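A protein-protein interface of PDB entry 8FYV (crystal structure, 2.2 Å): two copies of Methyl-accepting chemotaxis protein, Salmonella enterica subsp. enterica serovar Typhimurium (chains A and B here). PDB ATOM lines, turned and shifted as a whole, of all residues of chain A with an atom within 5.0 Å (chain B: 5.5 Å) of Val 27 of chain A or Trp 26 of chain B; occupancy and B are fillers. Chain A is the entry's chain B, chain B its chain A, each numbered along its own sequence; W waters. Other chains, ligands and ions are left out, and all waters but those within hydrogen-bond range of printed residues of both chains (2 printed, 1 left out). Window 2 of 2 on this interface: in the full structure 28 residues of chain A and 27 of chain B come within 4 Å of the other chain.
The side-chain amide nitrogen of Asn 23 of chain A sits at hydrogen-bond distance from the side-chain amide oxygen of Asn 23 of chain B, 2.9 Å away.
The side-chain amide nitrogen (NE2) of Gln 129 of chain B sits close to the side-chain amide nitrogen (NE2) of Gln 31 of chain A.
The side-chain amide oxygen (OD1) of Asn 23 of chain B lies within hydrogen-bond range of the side-chain hydroxyl (OH) of Tyr 136 of chain B (2.9 Å).
OE2 of Glu 28 of chain B lies within hydrogen-bond range of NE2 of Gln 31 of chain B (3.3 Å).
OH of Tyr 101 of chain B lies within hydrogen-bond range of OE1 of Gln 129 of chain B (2.6 Å).
The side-chain carboxylate of Glu 28 of chain A lies close to the side-chain amide oxygen of Gln 31 of chain A (3.5 Å).
NE1 of Trp 26 of chain A touches CG2 of Val 27 of chain B (3.5 Å).
Val 27 of chain A touches Trp 26 of chain B (CG1 to NE1, 3.6 Å).
Leu 30 of chain B touches Val 27 of chain A (CD1 to CG1, 3.98 Å).
Leu 30 of chain A touches Gln 31 of chain B.
CG of Gln 31 of chain A touches CD2 of Leu 30 of chain B, at 3.6 Å.
Gln 31 of chain A touches Glu 133 of chain B (NE2 to OE1, 3.5 Å).
Of the printed residues of chain B, Asn 23 of chain A touches Asn 23.
Of the printed residues of chain B, Gln 31 of chain A touches Leu 30, Gln 129 and Glu 133.
Thr 25 of chain B touches none of the printed residues of chain A.
Trp 26 of chain B touches just one residue of chain A: Val 27 (3.6 Å).
Phe 132 of chain B touches none of the printed residues of chain A.
The nearest residue of chain B that does not touch Val 27 of chain A is Glu 133 of chain B (4.7 Å).
The nearest residue of chain A that does not touch Trp 26 of chain B is Gln 31 of chain A (4.7 Å).
The nearest printed residue of chain A that does not touch Gln 31 of chain B is Trp 26 of chain A (4.04 Å).
Hydrophobic or aromatic side chains of chain A within 4 Å of the printed part of chain B: Trp 26, Val 27 and Leu 30.
Along chain A the printed residues that touch a printed residue of chain B span positions 23 to 31.
Of the 15 printed residues of chain B, 7 touch a printed residue of chain A.
Hydrophobic or aromatic side chains of chain B that line the printed part of chain A: Trp 26, Val 27 and Leu 30.
Among the printed residues, 8 pairs touch across the chains.
Among the printed residues, no Asp or Glu carboxylate lies within 4 Å of a Lys or Arg side-chain nitrogen of the other chain.
Asn 23 of chain A touches its own counterpart, Asn 23 of chain B.
Trp 26 of chain A touches Val 27 of chain B, and with the chains exchanged Val 27 of chain A touches Trp 26 of chain B.
Val 27 of chain A touches Leu 30 of chain B, but with the chains exchanged Leu 30 of chain A does not touch Val 27 of chain B (4.01 Å).
Leu 30 of chain A touches Gln 31 of chain B, and with the chains exchanged Gln 31 of chain A touches Leu 30 of chain B.
Positions printed for both chains: 23, 24, 25, 26, 27, 28, 29, 30 and 31.
Water W1 lies within hydrogen-bond range of OE1 of Glu 133 of chain B, NE2 of Gln 129 of chain B and NE2 of Gln 31 of chain A.
Water W2 bridges NE2 of Gln 31 of chain A (2.7 Å) and NE2 of Gln 129 of chain B (3.0 Å).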
ATOM      1  N   ASN A  23       1.994 -25.849   4.209  1.00  0.00           N
ATOM      2  CA  ASN A  23       1.614 -25.411   2.871  1.00  0.00           C
ATOM      3  C   ASN A  23       0.272 -24.692   2.878  1.00  0.00           C
ATOM      4  O   ASN A  23       0.052 -23.779   2.074  1.00  0.00           O
ATOM      5  CB  ASN A  23       1.566 -26.607   1.921  1.00  0.00           C
ATOM      6  CG  ASN A  23       1.068 -26.233   0.539  1.00  0.00           C
ATOM      7  OD1 ASN A  23      -0.078 -26.506   0.182  1.00  0.00           O
ATOM      8  ND2 ASN A  23       1.931 -25.600  -0.248  1.00  0.00           N
ATOM      9  N   ALA A  24      -0.638 -25.090   3.769  1.00  0.00           N
ATOM     10  CA  ALA A  24      -1.924 -24.406   3.859  1.00  0.00           C
ATOM     11  C   ALA A  24      -1.751 -22.979   4.361  1.00  0.00           C
ATOM     12  O   ALA A  24      -2.450 -22.065   3.908  1.00  0.00           O
ATOM     13  CB  ALA A  24      -2.870 -25.189   4.769  1.00  0.00           C
ATOM     14  N   THR A  25      -0.826 -22.768   5.301  1.00  0.00           N
ATOM     15  CA  THR A  25      -0.508 -21.412   5.740  1.00  0.00           C
ATOM     16  C   THR A  25       0.086 -20.600   4.596  1.00  0.00           C
ATOM     17  O   THR A  25      -0.308 -19.454   4.357  1.00  0.00           O
ATOM     18  CB  THR A  25       0.466 -21.456   6.919  1.00  0.00           C
ATOM     19  OG1 THR A  25       0.112 -22.528   7.801  1.00  0.00           O
ATOM     20  CG2 THR A  25       0.443 -20.139   7.684  1.00  0.00           C
ATOM     21  N   TRP A  26       1.048 -21.187   3.882  1.00  0.00           N
ATOM     22  CA  TRP A  26       1.655 -20.526   2.730  1.00  0.00           C
ATOM     23  C   TRP A  26       0.590 -20.065   1.744  1.00  0.00           C
ATOM     24  O   TRP A  26       0.591 -18.910   1.302  1.00  0.00           O
ATOM     25  CB  TRP A  26       2.647 -21.493   2.077  1.00  0.00           C
ATOM     26  CG  TRP A  26       3.342 -21.019   0.831  1.00  0.00           C
ATOM     27  CD1 TRP A  26       3.596 -21.761  -0.288  1.00  0.00           C
ATOM     28  CD2 TRP A  26       3.897 -19.721   0.583  1.00  0.00           C
ATOM     29  NE1 TRP A  26       4.264 -21.005  -1.218  1.00  0.00           N
ATOM     30  CE2 TRP A  26       4.461 -19.749  -0.710  1.00  0.00           C
ATOM     31  CE3 TRP A  26       3.969 -18.538   1.323  1.00  0.00           C
ATOM     32  CZ2 TRP A  26       5.086 -18.640  -1.277  1.00  0.00           C
ATOM     33  CZ3 TRP A  26       4.589 -17.437   0.756  1.00  0.00           C
ATOM     34  CH2 TRP A  26       5.140 -17.497  -0.531  1.00  0.00           C
ATOM     35  N   VAL A  27      -0.350 -20.952   1.411  1.00  0.00           N
ATOM     36  CA  VAL A  27      -1.387 -20.611   0.442  1.00  0.00           C
ATOM     37  C   VAL A  27      -2.264 -19.483   0.970  1.00  0.00           C
ATOM     38  O   VAL A  27      -2.610 -18.549   0.235  1.00  0.00           O
ATOM     39  CB  VAL A  27      -2.223 -21.859   0.099  1.00  0.00           C
ATOM     40  CG1 VAL A  27      -3.493 -21.464  -0.641  1.00  0.00           C
ATOM     41  CG2 VAL A  27      -1.401 -22.835  -0.724  1.00  0.00           C
ATOM     42  N   GLU A  28      -2.644 -19.551   2.248  1.00  0.00           N
ATOM     43  CA  GLU A  28      -3.536 -18.539   2.802  1.00  0.00           C
ATOM     44  C   GLU A  28      -2.853 -17.179   2.901  1.00  0.00           C
ATOM     45  O   GLU A  28      -3.513 -16.146   2.736  1.00  0.00           O
ATOM     46  CB  GLU A  28      -4.043 -18.984   4.173  1.00  0.00           C
ATOM     47  CG  GLU A  28      -5.526 -18.735   4.395  1.00  0.00           C
ATOM     48  CD  GLU A  28      -6.402 -19.496   3.416  1.00  0.00           C
ATOM     49  OE1 GLU A  28      -6.243 -20.730   3.308  1.00  0.00           O
ATOM     50  OE2 GLU A  28      -7.248 -18.858   2.755  1.00  0.00           O
ATOM     51  N   LEU A  29      -1.546 -17.154   3.171  1.00  0.00           N
ATOM     52  CA  LEU A  29      -0.817 -15.889   3.143  1.00  0.00           C
ATOM     53  C   LEU A  29      -0.884 -15.255   1.760  1.00  0.00           C
ATOM     54  O   LEU A  29      -1.070 -14.040   1.632  1.00  0.00           O
ATOM     55  CB  LEU A  29       0.638 -16.108   3.554  1.00  0.00           C
ATOM     56  CG  LEU A  29       0.894 -16.372   5.037  1.00  0.00           C
ATOM     57  CD1 LEU A  29       2.191 -17.143   5.221  1.00  0.00           C
ATOM     58  CD2 LEU A  29       0.927 -15.070   5.822  1.00  0.00           C
ATOM     59  N   LEU A  30      -0.735 -16.067   0.710  1.00  0.00           N
ATOM     60  CA  LEU A  30      -0.768 -15.533  -0.647  1.00  0.00           C
ATOM     61  C   LEU A  30      -2.142 -14.963  -0.981  1.00  0.00           C
ATOM     62  O   LEU A  30      -2.244 -13.878  -1.564  1.00  0.00           O
ATOM     63  CB  LEU A  30      -0.379 -16.624  -1.644  1.00  0.00           C
ATOM     64  CG  LEU A  30       1.075 -17.103  -1.592  1.00  0.00           C
ATOM     65  CD1 LEU A  30       1.256 -18.390  -2.391  1.00  0.00           C
ATOM     66  CD2 LEU A  30       2.016 -16.024  -2.101  1.00  0.00           C
ATOM     67  N   GLN A  31      -3.210 -15.677  -0.617  1.00  0.00           N
ATOM     68  CA  GLN A  31      -4.554 -15.184  -0.903  1.00  0.00           C
ATOM     69  C   GLN A  31      -4.861 -13.922  -0.107  1.00  0.00           C
ATOM     70  O   GLN A  31      -5.494 -12.993  -0.624  1.00  0.00           O
ATOM     71  CB  GLN A  31      -5.583 -16.275  -0.610  1.00  0.00           C
ATOM     72  CG  GLN A  31      -5.657 -17.341  -1.692  1.00  0.00           C
ATOM     73  CD  GLN A  31      -6.523 -18.521  -1.303  1.00  0.00           C
ATOM     74  OE1 GLN A  31      -6.115 -19.375  -0.515  1.00  0.00           O
ATOM     75  NE2 GLN A  31      -7.726 -18.581  -1.863  1.00  0.00           N
ATOM     76  N   LEU B  22       1.973 -30.110  -8.833  1.00  0.00           N
ATOM     77  CA  LEU B  22       0.738 -29.342  -8.959  1.00  0.00           C
ATOM     78  C   LEU B  22       0.668 -28.224  -7.926  1.00  0.00           C
ATOM     79  O   LEU B  22       0.085 -27.169  -8.197  1.00  0.00           O
ATOM     80  CB  LEU B  22      -0.475 -30.263  -8.830  1.00  0.00           C
ATOM     81  CG  LEU B  22      -1.837 -29.674  -9.215  1.00  0.00           C
ATOM     82  CD1 LEU B  22      -1.745 -28.794 -10.458  1.00  0.00           C
ATOM     83  CD2 LEU B  22      -2.864 -30.779  -9.422  1.00  0.00           C
ATOM     84  N   ASN B  23       1.252 -28.431  -6.743  1.00  0.00           N
ATOM     85  CA  ASN B  23       1.274 -27.368  -5.743  1.00  0.00           C
ATOM     86  C   ASN B  23       2.091 -26.176  -6.228  1.00  0.00           C
ATOM     87  O   ASN B  23       1.719 -25.021  -5.991  1.00  0.00           O
ATOM     88  CB  ASN B  23       1.837 -27.898  -4.425  1.00  0.00           C
ATOM     89  CG  ASN B  23       1.828 -26.850  -3.328  1.00  0.00           C
ATOM     90  OD1 ASN B  23       0.799 -26.602  -2.699  1.00  0.00           O
ATOM     91  ND2 ASN B  23       2.977 -26.224  -3.096  1.00  0.00           N
ATOM     92  N   ALA B  24       3.211 -26.435  -6.908  1.00  0.00           N
ATOM     93  CA  ALA B  24       4.028 -25.340  -7.423  1.00  0.00           C
ATOM     94  C   ALA B  24       3.280 -24.538  -8.479  1.00  0.00           C
ATOM     95  O   ALA B  24       3.473 -23.322  -8.586  1.00  0.00           O
ATOM     96  CB  ALA B  24       5.337 -25.883  -7.998  1.00  0.00           C
ATOM     97  N   THR B  25       2.435 -25.200  -9.273  1.00  0.00           N
ATOM     98  CA  THR B  25       1.556 -24.478 -10.188  1.00  0.00           C
ATOM     99  C   THR B  25       0.558 -23.626  -9.414  1.00  0.00           C
ATOM    100  O   THR B  25       0.382 -22.435  -9.699  1.00  0.00           O
ATOM    101  CB  THR B  25       0.825 -25.467 -11.099  1.00  0.00           C
ATOM    102  OG1 THR B  25       1.755 -26.430 -11.612  1.00  0.00           O
ATOM    103  CG2 THR B  25       0.156 -24.744 -12.261  1.00  0.00           C
ATOM    104  N   TRP B  26      -0.107 -24.228  -8.425  1.00  0.00           N
ATOM    105  CA  TRP B  26      -1.044 -23.502  -7.571  1.00  0.00           C
ATOM    106  C   TRP B  26      -0.397 -22.257  -6.978  1.00  0.00           C
ATOM    107  O   TRP B  26      -0.964 -21.159  -7.032  1.00  0.00           O
ATOM    108  CB  TRP B  26      -1.536 -24.451  -6.475  1.00  0.00           C
ATOM    109  CG  TRP B  26      -2.525 -23.907  -5.479  1.00  0.00           C
ATOM    110  CD1 TRP B  26      -2.610 -24.247  -4.158  1.00  0.00           C
ATOM    111  CD2 TRP B  26      -3.579 -22.965  -5.717  1.00  0.00           C
ATOM    112  NE1 TRP B  26      -3.642 -23.571  -3.559  1.00  0.00           N
ATOM    113  CE2 TRP B  26      -4.255 -22.778  -4.493  1.00  0.00           C
ATOM    114  CE3 TRP B  26      -4.017 -22.261  -6.842  1.00  0.00           C
ATOM    115  CZ2 TRP B  26      -5.339 -21.914  -4.363  1.00  0.00           C
ATOM    116  CZ3 TRP B  26      -5.095 -21.403  -6.710  1.00  0.00           C
ATOM    117  CH2 TRP B  26      -5.743 -21.237  -5.479  1.00  0.00           C
ATOM    118  N   VAL B  27       0.806 -22.408  -6.423  1.00  0.00           N
ATOM    119  CA  VAL B  27       1.467 -21.287  -5.765  1.00  0.00           C
ATOM    120  C   VAL B  27       1.802 -20.190  -6.769  1.00  0.00           C
ATOM    121  O   VAL B  27       1.642 -18.998  -6.482  1.00  0.00           O
ATOM    122  CB  VAL B  27       2.724 -21.779  -5.024  1.00  0.00           C
ATOM    123  CG1 VAL B  27       3.648 -20.615  -4.720  1.00  0.00           C
ATOM    124  CG2 VAL B  27       2.335 -22.508  -3.748  1.00  0.00           C
ATOM    125  N   GLU B  28       2.278 -20.570  -7.958  1.00  0.00           N
ATOM    126  CA  GLU B  28       2.669 -19.566  -8.942  1.00  0.00           C
ATOM    127  C   GLU B  28       1.460 -18.834  -9.512  1.00  0.00           C
ATOM    128  O   GLU B  28       1.560 -17.649  -9.848  1.00  0.00           O
ATOM    129  CB  GLU B  28       3.473 -20.216 -10.066  1.00  0.00           C
ATOM    130  CG  GLU B  28       4.868 -20.667  -9.650  1.00  0.00           C
ATOM    131  CD  GLU B  28       5.714 -19.530  -9.106  1.00  0.00           C
ATOM    132  OE1 GLU B  28       5.486 -18.370  -9.511  1.00  0.00           O
ATOM    133  OE2 GLU B  28       6.603 -19.796  -8.268  1.00  0.00           O
ATOM    134  N   LEU B  29       0.318 -19.514  -9.634  1.00  0.00           N
ATOM    135  CA  LEU B  29      -0.901 -18.831 -10.056  1.00  0.00           C
ATOM    136  C   LEU B  29      -1.282 -17.746  -9.057  1.00  0.00           C
ATOM    137  O   LEU B  29      -1.613 -16.618  -9.440  1.00  0.00           O
ATOM    138  CB  LEU B  29      -2.039 -19.839 -10.214  1.00  0.00           C
ATOM    139  CG  LEU B  29      -2.081 -20.602 -11.539  1.00  0.00           C
ATOM    140  CD1 LEU B  29      -2.846 -21.907 -11.381  1.00  0.00           C
ATOM    141  CD2 LEU B  29      -2.694 -19.743 -12.635  1.00  0.00           C
ATOM    142  N   LEU B  30      -1.238 -18.073  -7.763  1.00  0.00           N
ATOM    143  CA  LEU B  30      -1.566 -17.085  -6.741  1.00  0.00           C
ATOM    144  C   LEU B  30      -0.582 -15.923  -6.765  1.00  0.00           C
ATOM    145  O   LEU B  30      -0.982 -14.756  -6.671  1.00  0.00           O
ATOM    146  CB  LEU B  30      -1.583 -17.747  -5.363  1.00  0.00           C
ATOM    147  CG  LEU B  30      -2.720 -18.742  -5.124  1.00  0.00           C
ATOM    148  CD1 LEU B  30      -2.344 -19.739  -4.035  1.00  0.00           C
ATOM    149  CD2 LEU B  30      -4.009 -18.015  -4.769  1.00  0.00           C
ATOM    150  N   GLN B  31       0.710 -16.220  -6.892  1.00  0.00           N
ATOM    151  CA  GLN B  31       1.704 -15.154  -6.945  1.00  0.00           C
ATOM    152  C   GLN B  31       1.518 -14.281  -8.180  1.00  0.00           C
ATOM    153  O   GLN B  31       1.773 -13.073  -8.128  1.00  0.00           O
ATOM    154  CB  GLN B  31       3.109 -15.754  -6.913  1.00  0.00           C
ATOM    155  CG  GLN B  31       3.663 -15.896  -5.501  1.00  0.00           C
ATOM    156  CD  GLN B  31       4.926 -16.732  -5.423  1.00  0.00           C
ATOM    157  OE1 GLN B  31       5.803 -16.462  -4.605  1.00  0.00           O
ATOM    158  NE2 GLN B  31       5.017 -17.760  -6.259  1.00  0.00           N
ATOM    159  N   TYR B 101      -8.498 -20.639 -15.335  1.00  0.00           N
ATOM    160  CA  TYR B 101      -7.828 -19.721 -14.416  1.00  0.00           C
ATOM    161  C   TYR B 101      -6.572 -19.137 -15.053  1.00  0.00           C
ATOM    162  O   TYR B 101      -6.361 -17.919 -15.032  1.00  0.00           O
ATOM    163  CB  TYR B 101      -7.501 -20.448 -13.110  1.00  0.00           C
ATOM    164  CG  TYR B 101      -6.944 -19.571 -12.005  1.00  0.00           C
ATOM    165  CD1 TYR B 101      -7.128 -18.195 -12.011  1.00  0.00           C
ATOM    166  CD2 TYR B 101      -6.237 -20.130 -10.948  1.00  0.00           C
ATOM    167  CE1 TYR B 101      -6.619 -17.399 -10.998  1.00  0.00           C
ATOM    168  CE2 TYR B 101      -5.726 -19.345  -9.934  1.00  0.00           C
ATOM    169  CZ  TYR B 101      -5.919 -17.981  -9.963  1.00  0.00           C
ATOM    170  OH  TYR B 101      -5.409 -17.202  -8.951  1.00  0.00           O
ATOM    171  N   GLN B 129     -10.531 -18.981  -9.763  1.00  0.00           N
ATOM    172  CA  GLN B 129      -9.605 -19.523  -8.776  1.00  0.00           C
ATOM    173  C   GLN B 129     -10.313 -20.475  -7.821  1.00  0.00           C
ATOM    174  O   GLN B 129      -9.776 -21.537  -7.485  1.00  0.00           O
ATOM    175  CB  GLN B 129      -8.946 -18.380  -8.002  1.00  0.00           C
ATOM    176  CG  GLN B 129      -8.007 -18.827  -6.890  1.00  0.00           C
ATOM    177  CD  GLN B 129      -7.420 -17.658  -6.122  1.00  0.00           C
ATOM    178  OE1 GLN B 129      -6.618 -16.890  -6.654  1.00  0.00           O
ATOM    179  NE2 GLN B 129      -7.821 -17.516  -4.863  1.00  0.00           N
ATOM    180  N   PHE B 132     -10.754 -23.882  -9.453  1.00  0.00           N
ATOM    181  CA  PHE B 132      -9.529 -24.674  -9.487  1.00  0.00           C
ATOM    182  C   PHE B 132      -9.162 -25.183  -8.099  1.00  0.00           C
ATOM    183  O   PHE B 132      -8.756 -26.341  -7.944  1.00  0.00           O
ATOM    184  CB  PHE B 132      -8.382 -23.848 -10.066  1.00  0.00           C
ATOM    185  CG  PHE B 132      -7.043 -24.519  -9.950  1.00  0.00           C
ATOM    186  CD1 PHE B 132      -6.681 -25.524 -10.829  1.00  0.00           C
ATOM    187  CD2 PHE B 132      -6.152 -24.152  -8.956  1.00  0.00           C
ATOM    188  CE1 PHE B 132      -5.454 -26.147 -10.724  1.00  0.00           C
ATOM    189  CE2 PHE B 132      -4.923 -24.772  -8.846  1.00  0.00           C
ATOM    190  CZ  PHE B 132      -4.574 -25.772  -9.731  1.00  0.00           C
ATOM    191  N   GLU B 133      -9.292 -24.333  -7.078  1.00  0.00           N
ATOM    192  CA  GLU B 133      -8.956 -24.756  -5.724  1.00  0.00           C
ATOM    193  C   GLU B 133      -9.873 -25.872  -5.240  1.00  0.00           C
ATOM    194  O   GLU B 133      -9.452 -26.724  -4.449  1.00  0.00           O
ATOM    195  CB  GLU B 133      -9.026 -23.564  -4.770  1.00  0.00           C
ATOM    196  CG  GLU B 133      -8.665 -23.904  -3.334  1.00  0.00           C
ATOM    197  CD  GLU B 133      -8.582 -22.677  -2.449  1.00  0.00           C
ATOM    198  OE1 GLU B 133      -9.176 -21.639  -2.809  1.00  0.00           O
ATOM    199  OE2 GLU B 133      -7.921 -22.749  -1.391  1.00  0.00           O
ATOM    200  N   TYR B 136      -8.307 -28.972  -6.747  1.00  0.00           N
ATOM    201  CA  TYR B 136      -7.032 -29.230  -6.085  1.00  0.00           C
ATOM    202  C   TYR B 136      -7.246 -29.847  -4.708  1.00  0.00           C
ATOM    203  O   TYR B 136      -6.592 -30.831  -4.346  1.00  0.00           O
ATOM    204  CB  TYR B 136      -6.231 -27.931  -5.976  1.00  0.00           C
ATOM    205  CG  TYR B 136      -4.870 -28.092  -5.337  1.00  0.00           C
ATOM    206  CD1 TYR B 136      -3.933 -28.972  -5.864  1.00  0.00           C
ATOM    207  CD2 TYR B 136      -4.522 -27.366  -4.206  1.00  0.00           C
ATOM    208  CE1 TYR B 136      -2.686 -29.122  -5.282  1.00  0.00           C
ATOM    209  CE2 TYR B 136      -3.278 -27.510  -3.617  1.00  0.00           C
ATOM    210  CZ  TYR B 136      -2.365 -28.389  -4.159  1.00  0.00           C
ATOM    211  OH  TYR B 136      -1.126 -28.535  -3.577  1.00  0.00           O
HETATM  212  O   HOH W   1      -9.774 -19.540  -4.068  1.00  0.00           O
HETATM  213  O   HOH W   2      -8.380 -16.036  -2.365  1.00  0.00           O
